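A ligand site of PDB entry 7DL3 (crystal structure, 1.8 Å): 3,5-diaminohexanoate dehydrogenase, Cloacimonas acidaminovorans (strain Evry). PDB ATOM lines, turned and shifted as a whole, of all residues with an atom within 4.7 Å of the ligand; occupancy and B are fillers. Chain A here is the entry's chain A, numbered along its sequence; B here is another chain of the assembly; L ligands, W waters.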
ATOM      1  N   ASP A 177     -40.918  -1.597  -9.847  1.00  0.00           N
ATOM      2  CA  ASP A 177     -40.166  -0.715 -10.733  1.00  0.00           C
ATOM      3  C   ASP A 177     -39.191  -1.476 -11.630  1.00  0.00           C
ATOM      4  O   ASP A 177     -38.960  -1.074 -12.775  1.00  0.00           O
ATOM      5  CB  ASP A 177     -39.387   0.297  -9.883  1.00  0.00           C
ATOM      6  CG  ASP A 177     -38.671   1.339 -10.730  1.00  0.00           C
ATOM      7  OD1 ASP A 177     -37.482   1.631 -10.435  1.00  0.00           O
ATOM      8  OD2 ASP A 177     -39.244   1.820 -11.722  1.00  0.00           O
ATOM      9  N   VAL A 178     -38.576  -2.534 -11.108  1.00  0.00           N
ATOM     10  CA  VAL A 178     -37.530  -3.232 -11.852  1.00  0.00           C
ATOM     11  C   VAL A 178     -37.910  -4.685 -12.109  1.00  0.00           C
ATOM     12  O   VAL A 178     -37.054  -5.464 -12.515  1.00  0.00           O
ATOM     13  CB  VAL A 178     -36.178  -3.149 -11.119  1.00  0.00           C
ATOM     14  CG1 VAL A 178     -35.671  -1.708 -11.082  1.00  0.00           C
ATOM     15  CG2 VAL A 178     -36.267  -3.730  -9.714  1.00  0.00           C
ATOM     16  N   ALA A 181     -36.541  -7.031 -14.958  1.00  0.00           N
ATOM     17  CA  ALA A 181     -35.166  -7.487 -15.117  1.00  0.00           C
ATOM     18  C   ALA A 181     -34.991  -8.921 -14.653  1.00  0.00           C
ATOM     19  O   ALA A 181     -34.572  -9.769 -15.464  1.00  0.00           O
ATOM     20  CB  ALA A 181     -34.211  -6.520 -14.413  1.00  0.00           C
ATOM     21  N   GLY A 199     -23.023  -3.558 -13.465  1.00  0.00           N
ATOM     22  CA  GLY A 199     -23.822  -2.758 -12.562  1.00  0.00           C
ATOM     23  C   GLY A 199     -24.482  -3.614 -11.497  1.00  0.00           C
ATOM     24  O   GLY A 199     -25.646  -3.415 -11.140  1.00  0.00           O
ATOM     25  N   ASN A 201     -24.391  -4.051  -8.297  1.00  0.00           N
ATOM     26  CA  ASN A 201     -24.821  -3.603  -6.977  1.00  0.00           C
ATOM     27  C   ASN A 201     -26.151  -2.881  -6.991  1.00  0.00           C
ATOM     28  O   ASN A 201     -26.747  -2.649  -5.935  1.00  0.00           O
ATOM     29  CB  ASN A 201     -23.750  -2.668  -6.391  1.00  0.00           C
ATOM     30  CG  ASN A 201     -24.001  -2.287  -4.925  1.00  0.00           C
ATOM     31  OD1 ASN A 201     -24.204  -1.110  -4.592  1.00  0.00           O
ATOM     32  ND2 ASN A 201     -23.962  -3.276  -4.051  1.00  0.00           N
ATOM     33  N   GLY A 202     -26.688  -2.566  -8.173  1.00  0.00           N
ATOM     34  CA  GLY A 202     -27.872  -1.744  -8.246  1.00  0.00           C
ATOM     35  C   GLY A 202     -29.126  -2.502  -7.854  1.00  0.00           C
ATOM     36  O   GLY A 202     -29.120  -3.691  -7.534  1.00  0.00           O
ATOM     37  N   LYS A 203     -30.234  -1.774  -7.929  1.00  0.00           N
ATOM     38  CA  LYS A 203     -31.519  -2.323  -7.549  1.00  0.00           C
ATOM     39  C   LYS A 203     -31.903  -3.502  -8.427  1.00  0.00           C
ATOM     40  O   LYS A 203     -32.305  -4.566  -7.936  1.00  0.00           O
ATOM     41  CB  LYS A 203     -32.539  -1.198  -7.629  1.00  0.00           C
ATOM     42  CG  LYS A 203     -33.920  -1.496  -7.191  1.00  0.00           C
ATOM     43  CD  LYS A 203     -34.557  -0.124  -7.279  1.00  0.00           C
ATOM     44  CE  LYS A 203     -36.005  -0.145  -7.099  1.00  0.00           C
ATOM     45  NZ  LYS A 203     -36.566   1.002  -7.868  1.00  0.00           N
ATOM     46  N   SER A 204     -31.826  -3.319  -9.747  1.00  0.00           N
ATOM     47  CA  SER A 204     -32.091  -4.454 -10.630  1.00  0.00           C
ATOM     48  C   SER A 204     -30.930  -5.429 -10.617  1.00  0.00           C
ATOM     49  O   SER A 204     -31.134  -6.637 -10.763  1.00  0.00           O
ATOM     50  CB  SER A 204     -32.415  -3.974 -12.050  1.00  0.00           C
ATOM     51  OG  SER A 204     -31.348  -3.253 -12.619  1.00  0.00           O
ATOM     52  N   GLY A 205     -29.697  -4.920 -10.425  1.00  0.00           N
ATOM     53  CA  GLY A 205     -28.515  -5.769 -10.453  1.00  0.00           C
ATOM     54  C   GLY A 205     -28.533  -6.867  -9.401  1.00  0.00           C
ATOM     55  O   GLY A 205     -28.202  -8.021  -9.701  1.00  0.00           O
ATOM     56  N   ARG A 227     -17.743  -0.754  -9.874  1.00  0.00           N
ATOM     57  CA  ARG A 227     -16.626   0.187  -9.829  1.00  0.00           C
ATOM     58  C   ARG A 227     -16.206   0.522  -8.407  1.00  0.00           C
ATOM     59  O   ARG A 227     -15.316   1.349  -8.222  1.00  0.00           O
ATOM     60  CB  ARG A 227     -16.952   1.452 -10.639  1.00  0.00           C
ATOM     61  CG  ARG A 227     -18.092   2.288 -10.152  1.00  0.00           C
ATOM     62  CD  ARG A 227     -18.230   3.479 -11.101  1.00  0.00           C
ATOM     63  NE  ARG A 227     -19.538   4.106 -11.049  1.00  0.00           N
ATOM     64  CZ  ARG A 227     -19.908   5.113 -11.837  1.00  0.00           C
ATOM     65  NH1 ARG A 227     -19.062   5.595 -12.743  1.00  0.00           N
ATOM     66  NH2 ARG A 227     -21.122   5.617 -11.740  1.00  0.00           N
ATOM     67  N   TYR A 231     -18.880  -2.544  -2.762  1.00  0.00           N
ATOM     68  CA  TYR A 231     -20.004  -3.340  -3.257  1.00  0.00           C
ATOM     69  C   TYR A 231     -19.729  -4.837  -3.364  1.00  0.00           C
ATOM     70  O   TYR A 231     -20.655  -5.604  -3.644  1.00  0.00           O
ATOM     71  CB  TYR A 231     -20.415  -2.844  -4.645  1.00  0.00           C
ATOM     72  CG  TYR A 231     -20.805  -1.391  -4.715  1.00  0.00           C
ATOM     73  CD1 TYR A 231     -21.043  -0.634  -3.568  1.00  0.00           C
ATOM     74  CD2 TYR A 231     -20.945  -0.760  -5.947  1.00  0.00           C
ATOM     75  CE1 TYR A 231     -21.376   0.714  -3.668  1.00  0.00           C
ATOM     76  CE2 TYR A 231     -21.294   0.561  -6.045  1.00  0.00           C
ATOM     77  CZ  TYR A 231     -21.516   1.296  -4.920  1.00  0.00           C
ATOM     78  OH  TYR A 231     -21.874   2.618  -5.078  1.00  0.00           O
ATOM     79  N   ALA A 246     -14.250  -2.490 -12.127  1.00  0.00           N
ATOM     80  CA  ALA A 246     -13.990  -1.742 -13.361  1.00  0.00           C
ATOM     81  C   ALA A 246     -15.089  -0.708 -13.533  1.00  0.00           C
ATOM     82  O   ALA A 246     -16.227  -0.924 -13.106  1.00  0.00           O
ATOM     83  CB  ALA A 246     -13.946  -2.657 -14.596  1.00  0.00           C
ATOM     84  N   GLN A 247     -14.717   0.402 -14.169  1.00  0.00           N
ATOM     85  CA  GLN A 247     -15.718   1.293 -14.721  1.00  0.00           C
ATOM     86  C   GLN A 247     -16.415   0.593 -15.869  1.00  0.00           C
ATOM     87  O   GLN A 247     -15.763  -0.065 -16.689  1.00  0.00           O
ATOM     88  CB  GLN A 247     -15.081   2.610 -15.198  1.00  0.00           C
ATOM     89  CG  GLN A 247     -14.304   3.388 -14.141  1.00  0.00           C
ATOM     90  CD  GLN A 247     -15.233   4.258 -13.299  1.00  0.00           C
ATOM     91  OE1 GLN A 247     -16.335   4.625 -13.745  1.00  0.00           O
ATOM     92  NE2 GLN A 247     -14.801   4.564 -12.071  1.00  0.00           N
ATOM     93  N   ALA A 248     -17.738   0.732 -15.936  1.00  0.00           N
ATOM     94  CA  ALA A 248     -18.503   0.039 -16.963  1.00  0.00           C
ATOM     95  C   ALA A 248     -18.196   0.562 -18.359  1.00  0.00           C
ATOM     96  O   ALA A 248     -18.570  -0.078 -19.349  1.00  0.00           O
ATOM     97  CB  ALA A 248     -19.999   0.158 -16.663  1.00  0.00           C
ATOM     98  N   THR A 249     -17.530   1.712 -18.460  1.00  0.00           N
ATOM     99  CA  THR A 249     -17.072   2.297 -19.704  1.00  0.00           C
ATOM    100  C   THR A 249     -15.719   1.760 -20.164  1.00  0.00           C
ATOM    101  O   THR A 249     -15.231   2.179 -21.224  1.00  0.00           O
ATOM    102  CB  THR A 249     -16.993   3.817 -19.546  1.00  0.00           C
ATOM    103  OG1 THR A 249     -16.310   4.133 -18.322  1.00  0.00           O
ATOM    104  CG2 THR A 249     -18.392   4.425 -19.512  1.00  0.00           C
ATOM    105  N   VAL A 273     -27.266  -3.412 -16.550  1.00  0.00           N
ATOM    106  CA  VAL A 273     -28.243  -2.722 -15.715  1.00  0.00           C
ATOM    107  C   VAL A 273     -27.602  -1.496 -15.074  1.00  0.00           C
ATOM    108  O   VAL A 273     -27.937  -1.141 -13.931  1.00  0.00           O
ATOM    109  CB  VAL A 273     -28.828  -3.685 -14.652  1.00  0.00           C
ATOM    110  CG1 VAL A 273     -29.813  -4.700 -15.282  1.00  0.00           C
ATOM    111  CG2 VAL A 273     -27.722  -4.403 -13.890  1.00  0.00           C
ATOM    112  N   VAL A 274     -26.696  -0.822 -15.793  1.00  0.00           N
ATOM    113  CA  VAL A 274     -26.086   0.430 -15.339  1.00  0.00           C
ATOM    114  C   VAL A 274     -26.984   1.601 -15.718  1.00  0.00           C
ATOM    115  O   VAL A 274     -27.959   1.424 -16.454  1.00  0.00           O
ATOM    116  CB  VAL A 274     -24.687   0.670 -15.922  1.00  0.00           C
ATOM    117  CG1 VAL A 274     -23.710  -0.396 -15.472  1.00  0.00           C
ATOM    118  CG2 VAL A 274     -24.729   0.809 -17.439  1.00  0.00           C
ATOM    119  N   ASN A 275     -26.763   2.777 -15.121  1.00  0.00           N
ATOM    120  CA  ASN A 275     -27.536   3.936 -15.517  1.00  0.00           C
ATOM    121  C   ASN A 275     -26.650   4.988 -16.176  1.00  0.00           C
ATOM    122  O   ASN A 275     -26.927   6.188 -16.084  1.00  0.00           O
ATOM    123  CB  ASN A 275     -28.293   4.538 -14.331  1.00  0.00           C
ATOM    124  CG  ASN A 275     -27.371   4.874 -13.160  1.00  0.00           C
ATOM    125  OD1 ASN A 275     -26.168   4.670 -13.239  1.00  0.00           O
ATOM    126  ND2 ASN A 275     -27.926   5.422 -12.083  1.00  0.00           N
ATOM    127  N   THR A 276     -25.581   4.572 -16.857  1.00  0.00           N
ATOM    128  CA  THR A 276     -24.708   5.512 -17.536  1.00  0.00           C
ATOM    129  C   THR A 276     -24.480   5.099 -18.989  1.00  0.00           C
ATOM    130  O   THR A 276     -24.719   3.959 -19.381  1.00  0.00           O
ATOM    131  CB  THR A 276     -23.363   5.695 -16.820  1.00  0.00           C
ATOM    132  OG1 THR A 276     -22.807   4.430 -16.466  1.00  0.00           O
ATOM    133  CG2 THR A 276     -23.527   6.536 -15.570  1.00  0.00           C
ATOM    134  N   PHE A 296     -30.635  -3.478 -20.416  1.00  0.00           N
ATOM    135  CA  PHE A 296     -31.745  -2.937 -19.656  1.00  0.00           C
ATOM    136  C   PHE A 296     -31.667  -1.440 -19.437  1.00  0.00           C
ATOM    137  O   PHE A 296     -32.698  -0.798 -19.262  1.00  0.00           O
ATOM    138  CB  PHE A 296     -31.869  -3.593 -18.288  1.00  0.00           C
ATOM    139  CG  PHE A 296     -32.766  -4.747 -18.296  1.00  0.00           C
ATOM    140  CD1 PHE A 296     -32.261  -6.033 -18.390  1.00  0.00           C
ATOM    141  CD2 PHE A 296     -34.130  -4.554 -18.336  1.00  0.00           C
ATOM    142  CE1 PHE A 296     -33.108  -7.128 -18.445  1.00  0.00           C
ATOM    143  CE2 PHE A 296     -34.984  -5.642 -18.389  1.00  0.00           C
ATOM    144  CZ  PHE A 296     -34.473  -6.929 -18.444  1.00  0.00           C
ATOM    145  N   SER A 297     -30.494  -0.853 -19.518  1.00  0.00           N
ATOM    146  CA  SER A 297     -30.347   0.538 -19.139  1.00  0.00           C
ATOM    147  C   SER A 297     -31.030   1.414 -20.179  1.00  0.00           C
ATOM    148  O   SER A 297     -30.798   1.269 -21.385  1.00  0.00           O
ATOM    149  CB  SER A 297     -28.874   0.881 -19.064  1.00  0.00           C
ATOM    150  OG  SER A 297     -28.649   2.280 -19.059  1.00  0.00           O
ATOM    151  N   MET A 298     -31.814   2.385 -19.699  1.00  0.00           N
ATOM    152  CA  MET A 298     -32.420   3.366 -20.566  1.00  0.00           C
ATOM    153  C   MET A 298     -31.384   4.332 -21.125  1.00  0.00           C
ATOM    154  O   MET A 298     -31.732   5.180 -21.950  1.00  0.00           O
ATOM    155  CB  MET A 298     -33.510   4.118 -19.815  1.00  0.00           C
ATOM    156  CG  MET A 298     -34.748   3.266 -19.498  1.00  0.00           C
ATOM    157  SD  MET A 298     -35.576   2.644 -20.970  1.00  0.00           S
ATOM    158  CE  MET A 298     -36.522   4.055 -21.398  1.00  0.00           C
ATOM    159  N   ALA A 299     -30.137   4.248 -20.664  1.00  0.00           N
ATOM    160  CA  ALA A 299     -29.032   4.987 -21.237  1.00  0.00           C
ATOM    161  C   ALA A 299     -28.442   4.323 -22.493  1.00  0.00           C
ATOM    162  O   ALA A 299     -27.622   4.934 -23.161  1.00  0.00           O
ATOM    163  CB  ALA A 299     -27.926   5.191 -20.195  1.00  0.00           C
ATOM    164  N   GLY A 321     -33.860  -4.299 -23.740  1.00  0.00           N
ATOM    165  CA  GLY A 321     -34.515  -4.794 -22.538  1.00  0.00           C
ATOM    166  C   GLY A 321     -35.951  -4.360 -22.391  1.00  0.00           C
ATOM    167  O   GLY A 321     -36.251  -3.166 -22.307  1.00  0.00           O
ATOM    168  N   GLY A 323     -38.992  -3.962 -20.266  1.00  0.00           N
ATOM    169  CA  GLY A 323     -39.366  -3.839 -18.879  1.00  0.00           C
ATOM    170  C   GLY A 323     -40.614  -4.619 -18.478  1.00  0.00           C
ATOM    171  O   GLY A 323     -40.813  -4.861 -17.274  1.00  0.00           O
ATOM    172  N   TYR A 350     -34.690   0.135   0.479  1.00  0.00           N
ATOM    173  CA  TYR A 350     -35.869   0.724  -0.154  1.00  0.00           C
ATOM    174  C   TYR A 350     -37.168   0.679   0.641  1.00  0.00           C
ATOM    175  O   TYR A 350     -38.173   1.208   0.164  1.00  0.00           O
ATOM    176  CB  TYR A 350     -36.127   0.032  -1.505  1.00  0.00           C
ATOM    177  CG  TYR A 350     -34.889  -0.123  -2.336  1.00  0.00           C
ATOM    178  CD1 TYR A 350     -34.178   0.988  -2.757  1.00  0.00           C
ATOM    179  CD2 TYR A 350     -34.402  -1.392  -2.679  1.00  0.00           C
ATOM    180  CE1 TYR A 350     -33.034   0.864  -3.513  1.00  0.00           C
ATOM    181  CE2 TYR A 350     -33.250  -1.524  -3.427  1.00  0.00           C
ATOM    182  CZ  TYR A 350     -32.575  -0.402  -3.853  1.00  0.00           C
ATOM    183  OH  TYR A 350     -31.436  -0.519  -4.599  1.00  0.00           O
ATOM    184  N   GLU B 310     -43.614  -1.569 -23.185  1.00  0.00           N
ATOM    185  CA  GLU B 310     -44.083  -1.536 -21.797  1.00  0.00           C
ATOM    186  C   GLU B 310     -45.485  -0.929 -21.682  1.00  0.00           C
ATOM    187  O   GLU B 310     -46.346  -1.486 -20.988  1.00  0.00           O
ATOM    188  CB  GLU B 310     -43.068  -0.746 -20.954  1.00  0.00           C
ATOM    189  CG  GLU B 310     -43.556  -0.150 -19.633  1.00  0.00           C
ATOM    190  CD  GLU B 310     -42.569   0.843 -19.024  1.00  0.00           C
ATOM    191  OE1 GLU B 310     -41.334   0.650 -19.189  1.00  0.00           O
ATOM    192  OE2 GLU B 310     -43.051   1.833 -18.404  1.00  0.00           O
HETATM  193  P1  LIG L   1     -29.604   1.627  -9.821  1.00  0.00           P
HETATM  194  O1  LIG L   1     -30.194   0.926  -8.621  1.00  0.00           O
HETATM  195  O2  LIG L   1     -29.173   3.069  -9.753  1.00  0.00           O
HETATM  196  O3  LIG L   1     -28.453   0.669 -10.402  1.00  0.00           O
HETATM  197  C1  LIG L   1     -27.467   1.137 -11.318  1.00  0.00           C
HETATM  198  C2  LIG L   1     -26.145   0.464 -10.938  1.00  0.00           C
HETATM  199  O4  LIG L   1     -25.213   0.724 -11.991  1.00  0.00           O
HETATM  200  C3  LIG L   1     -25.555   1.102  -9.685  1.00  0.00           C
HETATM  201  O5  LIG L   1     -25.106   0.080  -8.787  1.00  0.00           O
HETATM  202  C4  LIG L   1     -24.357   1.917 -10.159  1.00  0.00           C
HETATM  203  O6  LIG L   1     -23.316   1.893  -9.163  1.00  0.00           O
HETATM  204  C5  LIG L   1     -23.985   1.154 -11.416  1.00  0.00           C
HETATM  205  N1  LIG L   1     -23.269   1.983 -12.419  1.00  0.00           N
HETATM  206  C6  LIG L   1     -23.780   3.018 -13.106  1.00  0.00           C
HETATM  207  N2  LIG L   1     -22.865   3.535 -13.951  1.00  0.00           N
HETATM  208  C7  LIG L   1     -21.730   2.817 -13.798  1.00  0.00           C
HETATM  209  C8  LIG L   1     -20.375   2.827 -14.370  1.00  0.00           C
HETATM  210  N3  LIG L   1     -20.043   3.737 -15.307  1.00  0.00           N
HETATM  211  N4  LIG L   1     -19.488   1.898 -13.944  1.00  0.00           N
HETATM  212  C9  LIG L   1     -19.821   0.989 -13.017  1.00  0.00           C
HETATM  213  N5  LIG L   1     -21.031   0.915 -12.436  1.00  0.00           N
HETATM  214  C10 LIG L   1     -22.007   1.788 -12.800  1.00  0.00           C
HETATM  215  O7  LIG L   1     -30.704   1.628 -11.011  1.00  0.00           O
HETATM  216  P2  LIG L   1     -31.784   0.472 -11.348  1.00  0.00           P
HETATM  217  O8  LIG L   1     -33.140   0.853 -10.799  1.00  0.00           O
HETATM  218  O9  LIG L   1     -31.246  -0.925 -11.186  1.00  0.00           O
HETATM  219  O10 LIG L   1     -31.830   0.733 -12.932  1.00  0.00           O
HETATM  220  C11 LIG L   1     -30.652   0.485 -13.716  1.00  0.00           C
HETATM  221  C12 LIG L   1     -30.951   0.834 -15.172  1.00  0.00           C
HETATM  222  O11 LIG L   1     -31.714  -0.224 -15.773  1.00  0.00           O
HETATM  223  C13 LIG L   1     -31.803   2.086 -15.374  1.00  0.00           C
HETATM  224  O12 LIG L   1     -31.420   2.665 -16.628  1.00  0.00           O
HETATM  225  C14 LIG L   1     -33.211   1.573 -15.542  1.00  0.00           C
HETATM  226  O13 LIG L   1     -33.952   2.489 -16.351  1.00  0.00           O
HETATM  227  C15 LIG L   1     -32.954   0.272 -16.268  1.00  0.00           C
HETATM  228  N6  LIG L   1     -33.997  -0.762 -16.123  1.00  0.00           N
HETATM  229  C16 LIG L   1     -35.151  -0.587 -16.798  1.00  0.00           C
HETATM  230  C17 LIG L   1     -36.158  -1.546 -16.706  1.00  0.00           C
HETATM  231  C18 LIG L   1     -37.446  -1.315 -17.452  1.00  0.00           C
HETATM  232  O14 LIG L   1     -38.511  -1.404 -16.852  1.00  0.00           O
HETATM  233  N7  LIG L   1     -37.384  -1.017 -18.758  1.00  0.00           N
HETATM  234  C19 LIG L   1     -35.958  -2.700 -15.948  1.00  0.00           C
HETATM  235  C20 LIG L   1     -34.752  -2.859 -15.270  1.00  0.00           C
HETATM  236  C21 LIG L   1     -33.787  -1.867 -15.385  1.00  0.00           C
HETATM  237  P3  LIG L   1     -22.480   3.201  -8.729  1.00  0.00           P
HETATM  238  O15 LIG L   1     -22.904   4.314  -9.670  1.00  0.00           O
HETATM  239  O16 LIG L   1     -22.835   3.435  -7.282  1.00  0.00           O
HETATM  240  O17 LIG L   1     -21.039   2.753  -8.937  1.00  0.00           O
HETATM  241  O   HOH W   1     -39.650  -3.552 -15.129  1.00  0.00           O
HETATM  242  O   HOH W   2     -20.738   0.069  -9.706  1.00  0.00           O
HETATM  243  O   HOH W   3     -30.356   1.633  -5.930  1.00  0.00           O
HETATM  244  O   HOH W   4     -28.865  -2.156 -11.246  1.00  0.00           O
HETATM  245  O   HOH W   5     -19.450   3.944  -7.197  1.00  0.00           O
HETATM  246  O   HOH W   6     -35.157  -1.378 -20.578  1.00  0.00           O
HETATM  247  O   HOH W   7     -30.524   5.328 -17.076  1.00  0.00           O
HETATM  248  O   HOH W   8     -24.906   1.058  -6.515  1.00  0.00           O
HETATM  249  O   HOH W   9     -33.676   2.838  -9.113  1.00  0.00           O
HETATM  250  O   HOH W  10     -17.564   5.093 -16.131  1.00  0.00           O
HETATM  251  O   HOH W  11     -35.351   1.904 -12.058  1.00  0.00           O
HETATM  252  O   HOH W  12     -23.156  -1.574  -9.573  1.00  0.00           O
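The side-chain hydroxyl (OG1) of Thr 276 lies within hydrogen-bond range of a nitrogen (N2) of the ligand. The side-chain hydroxyl (OG) of Ser 204 lies within hydrogen-bond range of an oxygen (O9) of the ligand. The backbone NH of Gly 202 sits at hydrogen-bond distance from an oxygen (O5) of the ligand, 3.1 Å away. An oxygen (O12) of the ligand lies within hydrogen-bond range of the backbone NH (N) of Met 298 (3.1 Å). O9 of the ligand sits at hydrogen-bond distance from N of Ser 204. The backbone NH of Lys 203 is in hydrogen-bond range of an oxygen (O1) of the ligand, at 2.8 Å. N of Ala 248 is in hydrogen-bond range of N4 of the ligand. An oxygen (O17) of the ligand is in salt-bridge range of the guanidinium group (NE) of Arg 227 (2.9 Å). The side-chain hydroxyl of Tyr 231 lies within hydrogen-bond range of an oxygen (O16) of the ligand, 2.5 Å away.
NZ of Lys 203 is in salt-bridge range of OD1 of Asp 177 (2.8 Å). The side-chain hydroxyl (OG) of Ser 297 lies close to the backbone carbonyl oxygen (O) of Val 274, at 2.8 Å. The backbone NH (N) of Ala 299 is in hydrogen-bond range of the side-chain hydroxyl (OG) of Ser 297 (2.9 Å). NH1 of Arg 227 sits at hydrogen-bond distance from OE1 of Gln 247 (3.1 Å).
A nitrogen (N6) of the ligand sits close to the backbone carbonyl oxygen (O) of Phe 296 (3.4 Å). Merely in contact with the ligand: Asn 275, Val 273, Gly 323, Val 274, Ser 297, Val 178, Asn 201, Gly 199, Ala 181 and Gln 247. 19 residues have an atom within 4 Å of the ligand: Val 178, Ala 181, Gly 199, Asn 201, Gly 202, Lys 203, Ser 204, Arg 227, Tyr 231, Gln 247, Ala 248, Val 273, Val 274, Asn 275, Thr 276, Phe 296, Ser 297, Met 298 and Gly 323. The nearest printed residue that does not touch the ligand is Ala 246 (4.1 Å).
Water W8 lies within hydrogen-bond range of O5 of the ligand (2.5 Å) and OD1 of Asn 201 (3.0 Å). Water W5 bridges O17 of the ligand (2.6 Å) and OH of Tyr 231 (3.5 Å). Water W12 lies within hydrogen-bond range of an oxygen (O5) of the ligand (2.7 Å), the backbone NH (N) of Asn 201 (3.0 Å) and the backbone carbonyl oxygen (O) of Gly 199 (3.5 Å). Water W4 lies within hydrogen-bond range of O9 of the ligand (2.7 Å), N of Gly 205 (3.0 Å), O of Val 273 (3.0 Å), OG of Ser 204 (3.0 Å) and O of Gly 199 (3.5 Å). Water W6 lies within hydrogen-bond range of the backbone carbonyl oxygen (O) of Gly 321 (2.7 Å), the backbone carbonyl oxygen (O) of Phe 296 (2.8 Å) and a nitrogen (N7) of the ligand (2.9 Å). Water W10 lies within hydrogen-bond range of OG1 of Thr 249 (2.7 Å), OE1 of Gln 247 (2.7 Å) and N3 of the ligand (2.9 Å).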
